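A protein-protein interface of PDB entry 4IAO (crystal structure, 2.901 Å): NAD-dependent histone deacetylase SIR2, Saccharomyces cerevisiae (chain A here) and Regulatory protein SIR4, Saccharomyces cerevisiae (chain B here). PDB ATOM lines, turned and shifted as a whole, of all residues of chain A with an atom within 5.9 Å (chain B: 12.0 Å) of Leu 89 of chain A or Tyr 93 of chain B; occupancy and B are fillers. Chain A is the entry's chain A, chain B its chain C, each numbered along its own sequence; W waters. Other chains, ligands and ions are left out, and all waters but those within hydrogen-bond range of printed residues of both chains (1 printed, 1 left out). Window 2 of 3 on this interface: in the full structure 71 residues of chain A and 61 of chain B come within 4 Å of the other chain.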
ATOM      1  N   LEU A  85     -27.938  12.517  11.590  1.00  0.00           N
ATOM      2  CA  LEU A  85     -28.385  11.975  12.872  1.00  0.00           C
ATOM      3  C   LEU A  85     -29.896  12.088  13.060  1.00  0.00           C
ATOM      4  O   LEU A  85     -30.506  13.076  12.636  1.00  0.00           O
ATOM      5  CB  LEU A  85     -27.664  12.673  14.025  1.00  0.00           C
ATOM      6  CG  LEU A  85     -26.206  12.261  14.224  1.00  0.00           C
ATOM      7  CD1 LEU A  85     -25.457  13.357  14.955  1.00  0.00           C
ATOM      8  CD2 LEU A  85     -26.121  10.941  14.981  1.00  0.00           C
ATOM      9  N   PRO A  86     -30.503  11.074  13.711  1.00  0.00           N
ATOM     10  CA  PRO A  86     -31.942  11.047  13.987  1.00  0.00           C
ATOM     11  C   PRO A  86     -32.378  12.248  14.814  1.00  0.00           C
ATOM     12  O   PRO A  86     -31.560  12.837  15.523  1.00  0.00           O
ATOM     13  CB  PRO A  86     -32.113   9.767  14.813  1.00  0.00           C
ATOM     14  CG  PRO A  86     -30.996   8.903  14.402  1.00  0.00           C
ATOM     15  CD  PRO A  86     -29.841   9.833  14.155  1.00  0.00           C
ATOM     16  N   GLU A  87     -33.655  12.605  14.721  1.00  0.00           N
ATOM     17  CA  GLU A  87     -34.199  13.727  15.481  1.00  0.00           C
ATOM     18  C   GLU A  87     -34.230  13.423  16.983  1.00  0.00           C
ATOM     19  O   GLU A  87     -34.375  14.325  17.810  1.00  0.00           O
ATOM     20  CB  GLU A  87     -35.595  14.087  14.965  1.00  0.00           C
ATOM     21  CG  GLU A  87     -35.659  14.325  13.457  1.00  0.00           C
ATOM     22  CD  GLU A  87     -34.909  15.574  13.018  1.00  0.00           C
ATOM     23  OE1 GLU A  87     -33.661  15.535  12.932  1.00  0.00           O
ATOM     24  OE2 GLU A  87     -35.572  16.600  12.755  1.00  0.00           O
ATOM     25  N   ASP A  88     -34.105  12.142  17.317  1.00  0.00           N
ATOM     26  CA  ASP A  88     -33.926  11.698  18.695  1.00  0.00           C
ATOM     27  C   ASP A  88     -33.050  10.447  18.699  1.00  0.00           C
ATOM     28  O   ASP A  88     -33.187   9.591  17.827  1.00  0.00           O
ATOM     29  CB  ASP A  88     -35.277  11.433  19.372  1.00  0.00           C
ATOM     30  CG  ASP A  88     -36.276  10.734  18.454  1.00  0.00           C
ATOM     31  OD1 ASP A  88     -35.855   9.908  17.614  1.00  0.00           O
ATOM     32  OD2 ASP A  88     -37.489  11.013  18.580  1.00  0.00           O
ATOM     33  N   LEU A  89     -32.154  10.329  19.674  1.00  0.00           N
ATOM     34  CA  LEU A  89     -31.132   9.289  19.587  1.00  0.00           C
ATOM     35  C   LEU A  89     -30.568   8.755  20.904  1.00  0.00           C
ATOM     36  O   LEU A  89     -31.052   9.071  21.992  1.00  0.00           O
ATOM     37  CB  LEU A  89     -29.982   9.780  18.701  1.00  0.00           C
ATOM     38  CG  LEU A  89     -29.475  11.216  18.880  1.00  0.00           C
ATOM     39  CD1 LEU A  89     -28.791  11.424  20.229  1.00  0.00           C
ATOM     40  CD2 LEU A  89     -28.537  11.577  17.739  1.00  0.00           C
ATOM     41  N   ASN A  90     -29.535   7.930  20.766  1.00  0.00           N
ATOM     42  CA  ASN A  90     -28.759   7.428  21.890  1.00  0.00           C
ATOM     43  C   ASN A  90     -27.266   7.607  21.600  1.00  0.00           C
ATOM     44  O   ASN A  90     -26.898   8.171  20.571  1.00  0.00           O
ATOM     45  CB  ASN A  90     -29.109   5.960  22.186  1.00  0.00           C
ATOM     46  CG  ASN A  90     -28.214   4.968  21.443  1.00  0.00           C
ATOM     47  OD1 ASN A  90     -27.694   4.020  22.036  1.00  0.00           O
ATOM     48  ND2 ASN A  90     -28.033   5.181  20.148  1.00  0.00           N
ATOM     49  N   SER A  91     -26.415   7.103  22.489  1.00  0.00           N
ATOM     50  CA  SER A  91     -24.971   7.300  22.379  1.00  0.00           C
ATOM     51  C   SER A  91     -24.291   6.341  21.396  1.00  0.00           C
ATOM     52  O   SER A  91     -23.075   6.409  21.188  1.00  0.00           O
ATOM     53  CB  SER A  91     -24.319   7.170  23.760  1.00  0.00           C
ATOM     54  OG  SER A  91     -24.617   5.916  24.352  1.00  0.00           O
ATOM     55  N   TYR A  93     -24.970   6.038  18.129  1.00  0.00           N
ATOM     56  CA  TYR A  93     -24.758   6.696  16.842  1.00  0.00           C
ATOM     57  C   TYR A  93     -23.365   7.311  16.786  1.00  0.00           C
ATOM     58  O   TYR A  93     -22.745   7.389  15.725  1.00  0.00           O
ATOM     59  CB  TYR A  93     -25.806   7.786  16.627  1.00  0.00           C
ATOM     60  CG  TYR A  93     -27.219   7.260  16.588  1.00  0.00           C
ATOM     61  CD1 TYR A  93     -27.798   6.852  15.392  1.00  0.00           C
ATOM     62  CD2 TYR A  93     -27.976   7.164  17.745  1.00  0.00           C
ATOM     63  CE1 TYR A  93     -29.092   6.362  15.352  1.00  0.00           C
ATOM     64  CE2 TYR A  93     -29.273   6.673  17.713  1.00  0.00           C
ATOM     65  CZ  TYR A  93     -29.825   6.276  16.514  1.00  0.00           C
ATOM     66  OH  TYR A  93     -31.114   5.797  16.487  1.00  0.00           O
ATOM     67  N   ASP A 140     -29.925   4.689  28.669  1.00  0.00           N
ATOM     68  CA  ASP A 140     -28.911   4.643  27.620  1.00  0.00           C
ATOM     69  C   ASP A 140     -28.029   3.392  27.733  1.00  0.00           C
ATOM     70  O   ASP A 140     -27.670   2.975  28.837  1.00  0.00           O
ATOM     71  CB  ASP A 140     -28.050   5.907  27.654  1.00  0.00           C
ATOM     72  CG  ASP A 140     -27.189   6.064  26.415  1.00  0.00           C
ATOM     73  OD1 ASP A 140     -26.066   5.507  26.388  1.00  0.00           O
ATOM     74  OD2 ASP A 140     -27.642   6.742  25.466  1.00  0.00           O
ATOM     75  N   LEU A 142     -24.819   2.739  26.612  1.00  0.00           N
ATOM     76  CA  LEU A 142     -23.395   2.914  26.897  1.00  0.00           C
ATOM     77  C   LEU A 142     -23.090   3.419  28.303  1.00  0.00           C
ATOM     78  O   LEU A 142     -23.915   4.083  28.932  1.00  0.00           O
ATOM     79  CB  LEU A 142     -22.752   3.835  25.859  1.00  0.00           C
ATOM     80  CG  LEU A 142     -22.431   3.153  24.530  1.00  0.00           C
ATOM     81  CD1 LEU A 142     -22.052   4.183  23.483  1.00  0.00           C
ATOM     82  CD2 LEU A 142     -21.315   2.126  24.712  1.00  0.00           C
ATOM     83  N   ALA A 143     -21.889   3.114  28.783  1.00  0.00           N
ATOM     84  CA  ALA A 143     -21.442   3.620  30.072  1.00  0.00           C
ATOM     85  C   ALA A 143     -21.145   5.111  29.954  1.00  0.00           C
ATOM     86  O   ALA A 143     -21.264   5.688  28.873  1.00  0.00           O
ATOM     87  CB  ALA A 143     -20.204   2.865  30.538  1.00  0.00           C
ATOM     88  N   LYS A 144     -20.767   5.735  31.065  1.00  0.00           N
ATOM     89  CA  LYS A 144     -20.424   7.155  31.066  1.00  0.00           C
ATOM     90  C   LYS A 144     -19.018   7.383  30.523  1.00  0.00           C
ATOM     91  O   LYS A 144     -18.789   8.291  29.721  1.00  0.00           O
ATOM     92  CB  LYS A 144     -20.547   7.736  32.473  1.00  0.00           C
ATOM     93  CG  LYS A 144     -21.947   7.653  33.055  1.00  0.00           C
ATOM     94  CD  LYS A 144     -22.916   8.544  32.297  1.00  0.00           C
ATOM     95  CE  LYS A 144     -24.293   8.516  32.943  1.00  0.00           C
ATOM     96  NZ  LYS A 144     -25.234   9.495  32.337  1.00  0.00           N
ATOM     97  N   THR A 147     -18.769   6.608  26.694  1.00  0.00           N
ATOM     98  CA  THR A 147     -19.497   7.671  25.998  1.00  0.00           C
ATOM     99  C   THR A 147     -18.630   8.922  25.794  1.00  0.00           C
ATOM    100  O   THR A 147     -18.747   9.617  24.780  1.00  0.00           O
ATOM    101  CB  THR A 147     -20.823   8.024  26.723  1.00  0.00           C
ATOM    102  OG1 THR A 147     -21.696   6.886  26.699  1.00  0.00           O
ATOM    103  CG2 THR A 147     -21.527   9.198  26.054  1.00  0.00           C
ATOM    104  N   THR B  80     -13.356  16.567  28.649  1.00  0.00           N
ATOM    105  CA  THR B  80     -13.753  15.489  29.553  1.00  0.00           C
ATOM    106  C   THR B  80     -14.556  16.037  30.735  1.00  0.00           C
ATOM    107  O   THR B  80     -15.556  15.446  31.150  1.00  0.00           O
ATOM    108  CB  THR B  80     -12.531  14.724  30.104  1.00  0.00           C
ATOM    109  OG1 THR B  80     -11.606  14.451  29.048  1.00  0.00           O
ATOM    110  CG2 THR B  80     -12.961  13.417  30.748  1.00  0.00           C
ATOM    111  N   ASN B  82     -16.124  19.068  30.715  1.00  0.00           N
ATOM    112  CA  ASN B  82     -17.321  19.692  30.159  1.00  0.00           C
ATOM    113  C   ASN B  82     -18.433  18.717  29.742  1.00  0.00           C
ATOM    114  O   ASN B  82     -19.618  19.055  29.806  1.00  0.00           O
ATOM    115  CB  ASN B  82     -16.945  20.588  28.982  1.00  0.00           C
ATOM    116  CG  ASN B  82     -17.739  21.874  28.956  1.00  0.00           C
ATOM    117  OD1 ASN B  82     -18.774  21.967  28.297  1.00  0.00           O
ATOM    118  ND2 ASN B  82     -17.260  22.875  29.683  1.00  0.00           N
ATOM    119  N   ILE B  83     -18.048  17.515  29.309  1.00  0.00           N
ATOM    120  CA  ILE B  83     -19.005  16.465  28.934  1.00  0.00           C
ATOM    121  C   ILE B  83     -19.625  15.806  30.168  1.00  0.00           C
ATOM    122  O   ILE B  83     -20.850  15.789  30.323  1.00  0.00           O
ATOM    123  CB  ILE B  83     -18.388  15.375  28.035  1.00  0.00           C
ATOM    124  CG1 ILE B  83     -17.827  15.977  26.750  1.00  0.00           C
ATOM    125  CG2 ILE B  83     -19.432  14.335  27.681  1.00  0.00           C
ATOM    126  CD1 ILE B  83     -17.102  14.968  25.893  1.00  0.00           C
ATOM    127  N   LEU B  84     -18.767  15.240  31.018  1.00  0.00           N
ATOM    128  CA  LEU B  84     -19.186  14.562  32.243  1.00  0.00           C
ATOM    129  C   LEU B  84     -20.164  15.405  33.059  1.00  0.00           C
ATOM    130  O   LEU B  84     -20.980  14.873  33.805  1.00  0.00           O
ATOM    131  CB  LEU B  84     -17.960  14.221  33.101  1.00  0.00           C
ATOM    132  CG  LEU B  84     -17.495  12.762  33.129  1.00  0.00           C
ATOM    133  CD1 LEU B  84     -17.500  12.194  31.731  1.00  0.00           C
ATOM    134  CD2 LEU B  84     -16.108  12.625  33.747  1.00  0.00           C
ATOM    135  N   TRP B  85     -20.078  16.722  32.914  1.00  0.00           N
ATOM    136  CA  TRP B  85     -20.979  17.633  33.610  1.00  0.00           C
ATOM    137  C   TRP B  85     -22.400  17.596  33.062  1.00  0.00           C
ATOM    138  O   TRP B  85     -23.358  17.403  33.810  1.00  0.00           O
ATOM    139  CB  TRP B  85     -20.452  19.059  33.525  1.00  0.00           C
ATOM    140  CG  TRP B  85     -21.242  20.016  34.338  1.00  0.00           C
ATOM    141  CD1 TRP B  85     -22.112  20.965  33.882  1.00  0.00           C
ATOM    142  CD2 TRP B  85     -21.247  20.116  35.762  1.00  0.00           C
ATOM    143  NE1 TRP B  85     -22.652  21.658  34.939  1.00  0.00           N
ATOM    144  CE2 TRP B  85     -22.136  21.154  36.105  1.00  0.00           C
ATOM    145  CE3 TRP B  85     -20.581  19.429  36.783  1.00  0.00           C
ATOM    146  CZ2 TRP B  85     -22.376  21.524  37.426  1.00  0.00           C
ATOM    147  CZ3 TRP B  85     -20.819  19.798  38.093  1.00  0.00           C
ATOM    148  CH2 TRP B  85     -21.709  20.836  38.404  1.00  0.00           C
ATOM    149  N   ARG B  86     -22.533  17.793  31.756  1.00  0.00           N
ATOM    150  CA  ARG B  86     -23.848  17.845  31.134  1.00  0.00           C
ATOM    151  C   ARG B  86     -24.471  16.448  31.047  1.00  0.00           C
ATOM    152  O   ARG B  86     -25.679  16.306  30.868  1.00  0.00           O
ATOM    153  CB  ARG B  86     -23.758  18.493  29.749  1.00  0.00           C
ATOM    154  CG  ARG B  86     -25.047  19.162  29.307  1.00  0.00           C
ATOM    155  CD  ARG B  86     -24.883  19.926  28.001  1.00  0.00           C
ATOM    156  NE  ARG B  86     -26.112  20.635  27.645  1.00  0.00           N
ATOM    157  CZ  ARG B  86     -26.257  21.399  26.567  1.00  0.00           C
ATOM    158  NH1 ARG B  86     -25.248  21.561  25.720  1.00  0.00           N
ATOM    159  NH2 ARG B  86     -27.417  22.003  26.336  1.00  0.00           N
ATOM    160  N   ILE B  87     -23.628  15.425  31.143  1.00  0.00           N
ATOM    161  CA  ILE B  87     -24.080  14.038  31.067  1.00  0.00           C
ATOM    162  C   ILE B  87     -24.595  13.360  32.346  1.00  0.00           C
ATOM    163  O   ILE B  87     -25.669  12.758  32.334  1.00  0.00           O
ATOM    164  CB  ILE B  87     -22.988  13.151  30.424  1.00  0.00           C
ATOM    165  CG1 ILE B  87     -22.928  13.419  28.921  1.00  0.00           C
ATOM    166  CG2 ILE B  87     -23.232  11.677  30.701  1.00  0.00           C
ATOM    167  CD1 ILE B  87     -24.291  13.531  28.269  1.00  0.00           C
ATOM    168  N   ALA B  88     -23.857  13.495  33.446  1.00  0.00           N
ATOM    169  CA  ALA B  88     -24.025  12.609  34.609  1.00  0.00           C
ATOM    170  C   ALA B  88     -25.422  12.579  35.229  1.00  0.00           C
ATOM    171  O   ALA B  88     -25.826  11.567  35.801  1.00  0.00           O
ATOM    172  CB  ALA B  88     -22.980  12.911  35.680  1.00  0.00           C
ATOM    173  N   ASP B  89     -26.156  13.678  35.104  1.00  0.00           N
ATOM    174  CA  ASP B  89     -27.486  13.762  35.700  1.00  0.00           C
ATOM    175  C   ASP B  89     -28.579  13.140  34.825  1.00  0.00           C
ATOM    176  O   ASP B  89     -29.756  13.162  35.191  1.00  0.00           O
ATOM    177  CB  ASP B  89     -27.835  15.215  36.057  1.00  0.00           C
ATOM    178  CG  ASP B  89     -27.291  15.636  37.424  1.00  0.00           C
ATOM    179  OD1 ASP B  89     -26.899  14.746  38.213  1.00  0.00           O
ATOM    180  OD2 ASP B  89     -27.265  16.855  37.714  1.00  0.00           O
ATOM    181  N   LYS B  90     -28.193  12.577  33.681  1.00  0.00           N
ATOM    182  CA  LYS B  90     -29.162  12.036  32.724  1.00  0.00           C
ATOM    183  C   LYS B  90     -28.781  10.657  32.164  1.00  0.00           C
ATOM    184  O   LYS B  90     -27.635  10.433  31.775  1.00  0.00           O
ATOM    185  CB  LYS B  90     -29.368  13.028  31.571  1.00  0.00           C
ATOM    186  CG  LYS B  90     -29.883  14.395  32.008  1.00  0.00           C
ATOM    187  CD  LYS B  90     -31.225  14.277  32.722  1.00  0.00           C
ATOM    188  CE  LYS B  90     -31.497  15.483  33.611  1.00  0.00           C
ATOM    189  NZ  LYS B  90     -32.764  15.320  34.374  1.00  0.00           N
ATOM    190  N   THR B  91     -29.743   9.733  32.147  1.00  0.00           N
ATOM    191  CA  THR B  91     -29.569   8.435  31.480  1.00  0.00           C
ATOM    192  C   THR B  91     -30.201   8.401  30.076  1.00  0.00           C
ATOM    193  O   THR B  91     -30.213   7.363  29.405  1.00  0.00           O
ATOM    194  CB  THR B  91     -30.090   7.255  32.332  1.00  0.00           C
ATOM    195  OG1 THR B  91     -29.880   7.533  33.722  1.00  0.00           O
ATOM    196  CG2 THR B  91     -29.360   5.961  31.966  1.00  0.00           C
ATOM    197  N   THR B  92     -30.761   9.531  29.651  1.00  0.00           N
ATOM    198  CA  THR B  92     -31.198   9.683  28.264  1.00  0.00           C
ATOM    199  C   THR B  92     -30.644  10.970  27.640  1.00  0.00           C
ATOM    200  O   THR B  92     -31.052  12.076  28.004  1.00  0.00           O
ATOM    201  CB  THR B  92     -32.737   9.666  28.150  1.00  0.00           C
ATOM    202  OG1 THR B  92     -33.299  10.585  29.096  1.00  0.00           O
ATOM    203  CG2 THR B  92     -33.277   8.267  28.428  1.00  0.00           C
ATOM    204  N   TYR B  93     -29.725  10.813  26.690  1.00  0.00           N
ATOM    205  CA  TYR B  93     -29.092  11.951  26.025  1.00  0.00           C
ATOM    206  C   TYR B  93     -30.003  12.534  24.945  1.00  0.00           C
ATOM    207  O   TYR B  93     -30.897  11.851  24.443  1.00  0.00           O
ATOM    208  CB  TYR B  93     -27.729  11.563  25.440  1.00  0.00           C
ATOM    209  CG  TYR B  93     -26.888  10.689  26.350  1.00  0.00           C
ATOM    210  CD1 TYR B  93     -26.800  10.939  27.719  1.00  0.00           C
ATOM    211  CD2 TYR B  93     -26.190   9.603  25.837  1.00  0.00           C
ATOM    212  CE1 TYR B  93     -26.035  10.128  28.546  1.00  0.00           C
ATOM    213  CE2 TYR B  93     -25.421   8.793  26.653  1.00  0.00           C
ATOM    214  CZ  TYR B  93     -25.347   9.054  28.004  1.00  0.00           C
ATOM    215  OH  TYR B  93     -24.581   8.231  28.802  1.00  0.00           O
ATOM    216  N   ASP B  94     -29.761  13.789  24.580  1.00  0.00           N
ATOM    217  CA  ASP B  94     -30.633  14.508  23.658  1.00  0.00           C
ATOM    218  C   ASP B  94     -29.918  14.761  22.321  1.00  0.00           C
ATOM    219  O   ASP B  94     -28.741  14.433  22.163  1.00  0.00           O
ATOM    220  CB  ASP B  94     -31.066  15.827  24.324  1.00  0.00           C
ATOM    221  CG  ASP B  94     -32.026  16.648  23.474  1.00  0.00           C
ATOM    222  OD1 ASP B  94     -32.085  17.881  23.673  1.00  0.00           O
ATOM    223  OD2 ASP B  94     -32.713  16.069  22.606  1.00  0.00           O
ATOM    224  N   LYS B  95     -30.638  15.334  21.362  1.00  0.00           N
ATOM    225  CA  LYS B  95     -30.065  15.696  20.075  1.00  0.00           C
ATOM    226  C   LYS B  95     -29.212  16.937  20.260  1.00  0.00           C
ATOM    227  O   LYS B  95     -27.988  16.875  20.166  1.00  0.00           O
ATOM    228  CB  LYS B  95     -31.171  15.966  19.049  1.00  0.00           C
ATOM    229  CG  LYS B  95     -30.694  16.650  17.768  1.00  0.00           C
ATOM    230  CD  LYS B  95     -31.844  16.923  16.807  1.00  0.00           C
ATOM    231  CE  LYS B  95     -31.364  17.647  15.555  1.00  0.00           C
ATOM    232  NZ  LYS B  95     -32.435  17.763  14.521  1.00  0.00           N
ATOM    233  N   GLU B  96     -29.871  18.055  20.554  1.00  0.00           N
ATOM    234  CA  GLU B  96     -29.208  19.341  20.745  1.00  0.00           C
ATOM    235  C   GLU B  96     -28.131  19.256  21.825  1.00  0.00           C
ATOM    236  O   GLU B  96     -27.172  20.024  21.819  1.00  0.00           O
ATOM    237  CB  GLU B  96     -30.239  20.408  21.112  1.00  0.00           C
ATOM    238  CG  GLU B  96     -31.583  20.201  20.436  1.00  0.00           C
ATOM    239  CD  GLU B  96     -32.724  20.837  21.205  1.00  0.00           C
ATOM    240  OE1 GLU B  96     -32.509  21.909  21.809  1.00  0.00           O
ATOM    241  OE2 GLU B  96     -33.835  20.257  21.209  1.00  0.00           O
ATOM    242  N   THR B  97     -28.311  18.339  22.770  1.00  0.00           N
ATOM    243  CA  THR B  97     -27.269  18.041  23.745  1.00  0.00           C
ATOM    244  C   THR B  97     -26.000  17.522  23.080  1.00  0.00           C
ATOM    245  O   THR B  97     -24.976  18.206  23.075  1.00  0.00           O
ATOM    246  CB  THR B  97     -27.750  17.053  24.819  1.00  0.00           C
ATOM    247  OG1 THR B  97     -28.767  17.677  25.613  1.00  0.00           O
ATOM    248  CG2 THR B  97     -26.598  16.645  25.722  1.00  0.00           C
ATOM    249  N   ILE B  98     -26.074  16.321  22.509  1.00  0.00           N
ATOM    250  CA  ILE B  98     -24.896  15.688  21.913  1.00  0.00           C
ATOM    251  C   ILE B  98     -24.284  16.470  20.747  1.00  0.00           C
ATOM    252  O   ILE B  98     -23.061  16.518  20.613  1.00  0.00           O
ATOM    253  CB  ILE B  98     -25.166  14.232  21.485  1.00  0.00           C
ATOM    254  CG1 ILE B  98     -25.578  13.400  22.694  1.00  0.00           C
ATOM    255  CG2 ILE B  98     -23.927  13.620  20.852  1.00  0.00           C
ATOM    256  CD1 ILE B  98     -25.438  11.910  22.476  1.00  0.00           C
ATOM    257  N   THR B  99     -25.115  17.092  19.912  1.00  0.00           N
ATOM    258  CA  THR B  99     -24.578  17.915  18.830  1.00  0.00           C
ATOM    259  C   THR B  99     -23.702  19.009  19.419  1.00  0.00           C
ATOM    260  O   THR B  99     -22.527  19.131  19.064  1.00  0.00           O
ATOM    261  CB  THR B  99     -25.672  18.566  17.946  1.00  0.00           C
ATOM    262  OG1 THR B  99     -26.384  19.563  18.690  1.00  0.00           O
ATOM    263  CG2 THR B  99     -26.633  17.519  17.413  1.00  0.00           C
ATOM    264  N   ASP B 100     -24.272  19.776  20.342  1.00  0.00           N
ATOM    265  CA  ASP B 100     -23.543  20.860  20.996  1.00  0.00           C
ATOM    266  C   ASP B 100     -22.355  20.324  21.789  1.00  0.00           C
ATOM    267  O   ASP B 100     -21.380  21.038  22.021  1.00  0.00           O
ATOM    268  CB  ASP B 100     -24.471  21.675  21.901  1.00  0.00           C
ATOM    269  CG  ASP B 100     -25.500  22.473  21.117  1.00  0.00           C
ATOM    270  OD1 ASP B 100     -25.869  22.044  20.001  1.00  0.00           O
ATOM    271  OD2 ASP B 100     -25.942  23.529  21.620  1.00  0.00           O
ATOM    272  N   LEU B 101     -22.434  19.064  22.195  1.00  0.00           N
ATOM    273  CA  LEU B 101     -21.321  18.436  22.889  1.00  0.00           C
ATOM    274  C   LEU B 101     -20.184  18.114  21.914  1.00  0.00           C
ATOM    275  O   LEU B 101     -19.009  18.213  22.268  1.00  0.00           O
ATOM    276  CB  LEU B 101     -21.789  17.182  23.627  1.00  0.00           C
ATOM    277  CG  LEU B 101     -21.080  16.851  24.943  1.00  0.00           C
ATOM    278  CD1 LEU B 101     -20.770  18.114  25.726  1.00  0.00           C
ATOM    279  CD2 LEU B 101     -21.942  15.923  25.777  1.00  0.00           C
ATOM    280  N   ILE B 102     -20.535  17.740  20.686  1.00  0.00           N
ATOM    281  CA  ILE B 102     -19.536  17.481  19.656  1.00  0.00           C
ATOM    282  C   ILE B 102     -18.942  18.779  19.121  1.00  0.00           C
ATOM    283  O   ILE B 102     -17.721  18.933  19.060  1.00  0.00           O
ATOM    284  CB  ILE B 102     -20.140  16.716  18.460  1.00  0.00           C
ATOM    285  CG1 ILE B 102     -20.772  15.404  18.918  1.00  0.00           C
ATOM    286  CG2 ILE B 102     -19.076  16.442  17.402  1.00  0.00           C
ATOM    287  CD1 ILE B 102     -19.808  14.475  19.583  1.00  0.00           C
ATOM    288  N   GLU B 103     -19.819  19.714  18.758  1.00  0.00           N
ATOM    289  CA  GLU B 103     -19.432  20.928  18.034  1.00  0.00           C
ATOM    290  C   GLU B 103     -18.447  21.833  18.771  1.00  0.00           C
ATOM    291  O   GLU B 103     -17.863  22.735  18.168  1.00  0.00           O
ATOM    292  CB  GLU B 103     -20.667  21.747  17.652  1.00  0.00           C
ATOM    293  CG  GLU B 103     -21.536  21.120  16.581  1.00  0.00           C
ATOM    294  CD  GLU B 103     -22.603  22.074  16.071  1.00  0.00           C
ATOM    295  OE1 GLU B 103     -23.624  21.593  15.530  1.00  0.00           O
ATOM    296  OE2 GLU B 103     -22.416  23.304  16.208  1.00  0.00           O
HETATM  297  O   HOH W   1     -29.321   8.650  25.373  1.00  0.00           O
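The side-chain amino group of Lys 144 of chain A sits at hydrogen-bond distance from the backbone carbonyl oxygen of Ile 87 of chain B (3.3 Å).
NZ of Lys 95 of chain B is in salt-bridge range of OE1 of Glu 87 of chain A (3.0 Å).
The side-chain amino group of Lys 144 of chain A sits at hydrogen-bond distance from the backbone carbonyl oxygen of Lys 90 of chain B (2.6 Å).
N of Asp 140 of chain A sits at hydrogen-bond distance from O of Thr 91 of chain B, 2.8 Å away.
Hydrophobic or aromatic side chains of chain A within 4 Å of the printed part of chain B: Leu 89.
Printed residues of chain B that touch a printed residue of chain A: Ile 87, Lys 90, Thr 91, Tyr 93, Asp 94 and Lys 95.
Among the printed residues, 10 pairs touch across the chains.
Among the printed residues, Asp or Glu carboxylates within 4 Å of a Lys or Arg side-chain nitrogen of the other chain: Glu 87 of chain A with Lys 95 of chain B (3.0 Å).
Leu 85 of chain A touches none of the printed residues of chain B.
No residue of chain B comes within 4 Å of Pro 86 of chain A.
Of the printed residues of chain B, Glu 87 of chain A touches Lys 95.
Of chain B, only Tyr 93 (3.7 Å) and Asp 94 (3.6 Å) come within 4 Å of Leu 89 of chain A.
No residue of chain B comes within 4 Å of Tyr 93 of chain A.
Asp 140 of chain A touches just these residues of chain B: Thr 91 (2.8 Å) and Tyr 93 (3.2 Å).
No residue of chain B comes within 4 Å of Ala 143 of chain A.
Of chain B, only Ile 87 (3.3 Å), Lys 90 (2.6 Å) and Tyr 93 (3.8 Å) come within 4 Å of Lys 144 of chain A.
Of chain B, only Tyr 93 (3.8 Å) comes within 4 Å of Thr 147 of chain A.
Of the printed residues of chain A, Asp 94 of chain B touches Leu 89.
Of the printed residues of chain A, Lys 95 of chain B touches Glu 87 (3.0 Å).
The nearest printed residue of chain A that does not touch Tyr 93 of chain B is Ala 143 of chain A (4.2 Å).
OD1 of Asp 140 of chain A sits at hydrogen-bond distance from OG of Ser 91 of chain A (2.5 Å).
The backbone carbonyl oxygen of Lys 95 of chain B sits close to the side-chain hydroxyl of Thr 99 of chain B (3.5 Å).
The side-chain carboxylate (OD1) of Asp 140 of chain A is in hydrogen-bond range of the backbone NH (N) of Leu 142 of chain A, 3.0 Å away.
The backbone carbonyl oxygen (O) of Ala 143 of chain A is in hydrogen-bond range of the side-chain hydroxyl (OG1) of Thr 147 of chain A, at 2.5 Å.
Water W1 lies within hydrogen-bond range of the side-chain carboxylate (OD2) of Asp 140 of chain A (2.5 Å) and the backbone NH (N) of Tyr 93 of chain B (2.6 Å).
O of Leu 89 of chain A touches O of Tyr 93 of chain B, 3.7 Å away.
Asp 94 of chain B touches Leu 89 of chain A.
Tyr 93 of chain B touches Ser 91 of chain A.
Asp 140 of chain A touches Tyr 93 of chain B (OD2 to CD2, 3.2 Å).
Lys 144 of chain A touches Tyr 93 of chain B.
Tyr 93 of chain B touches Thr 147 of chain A (OH to OG1, 3.8 Å).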
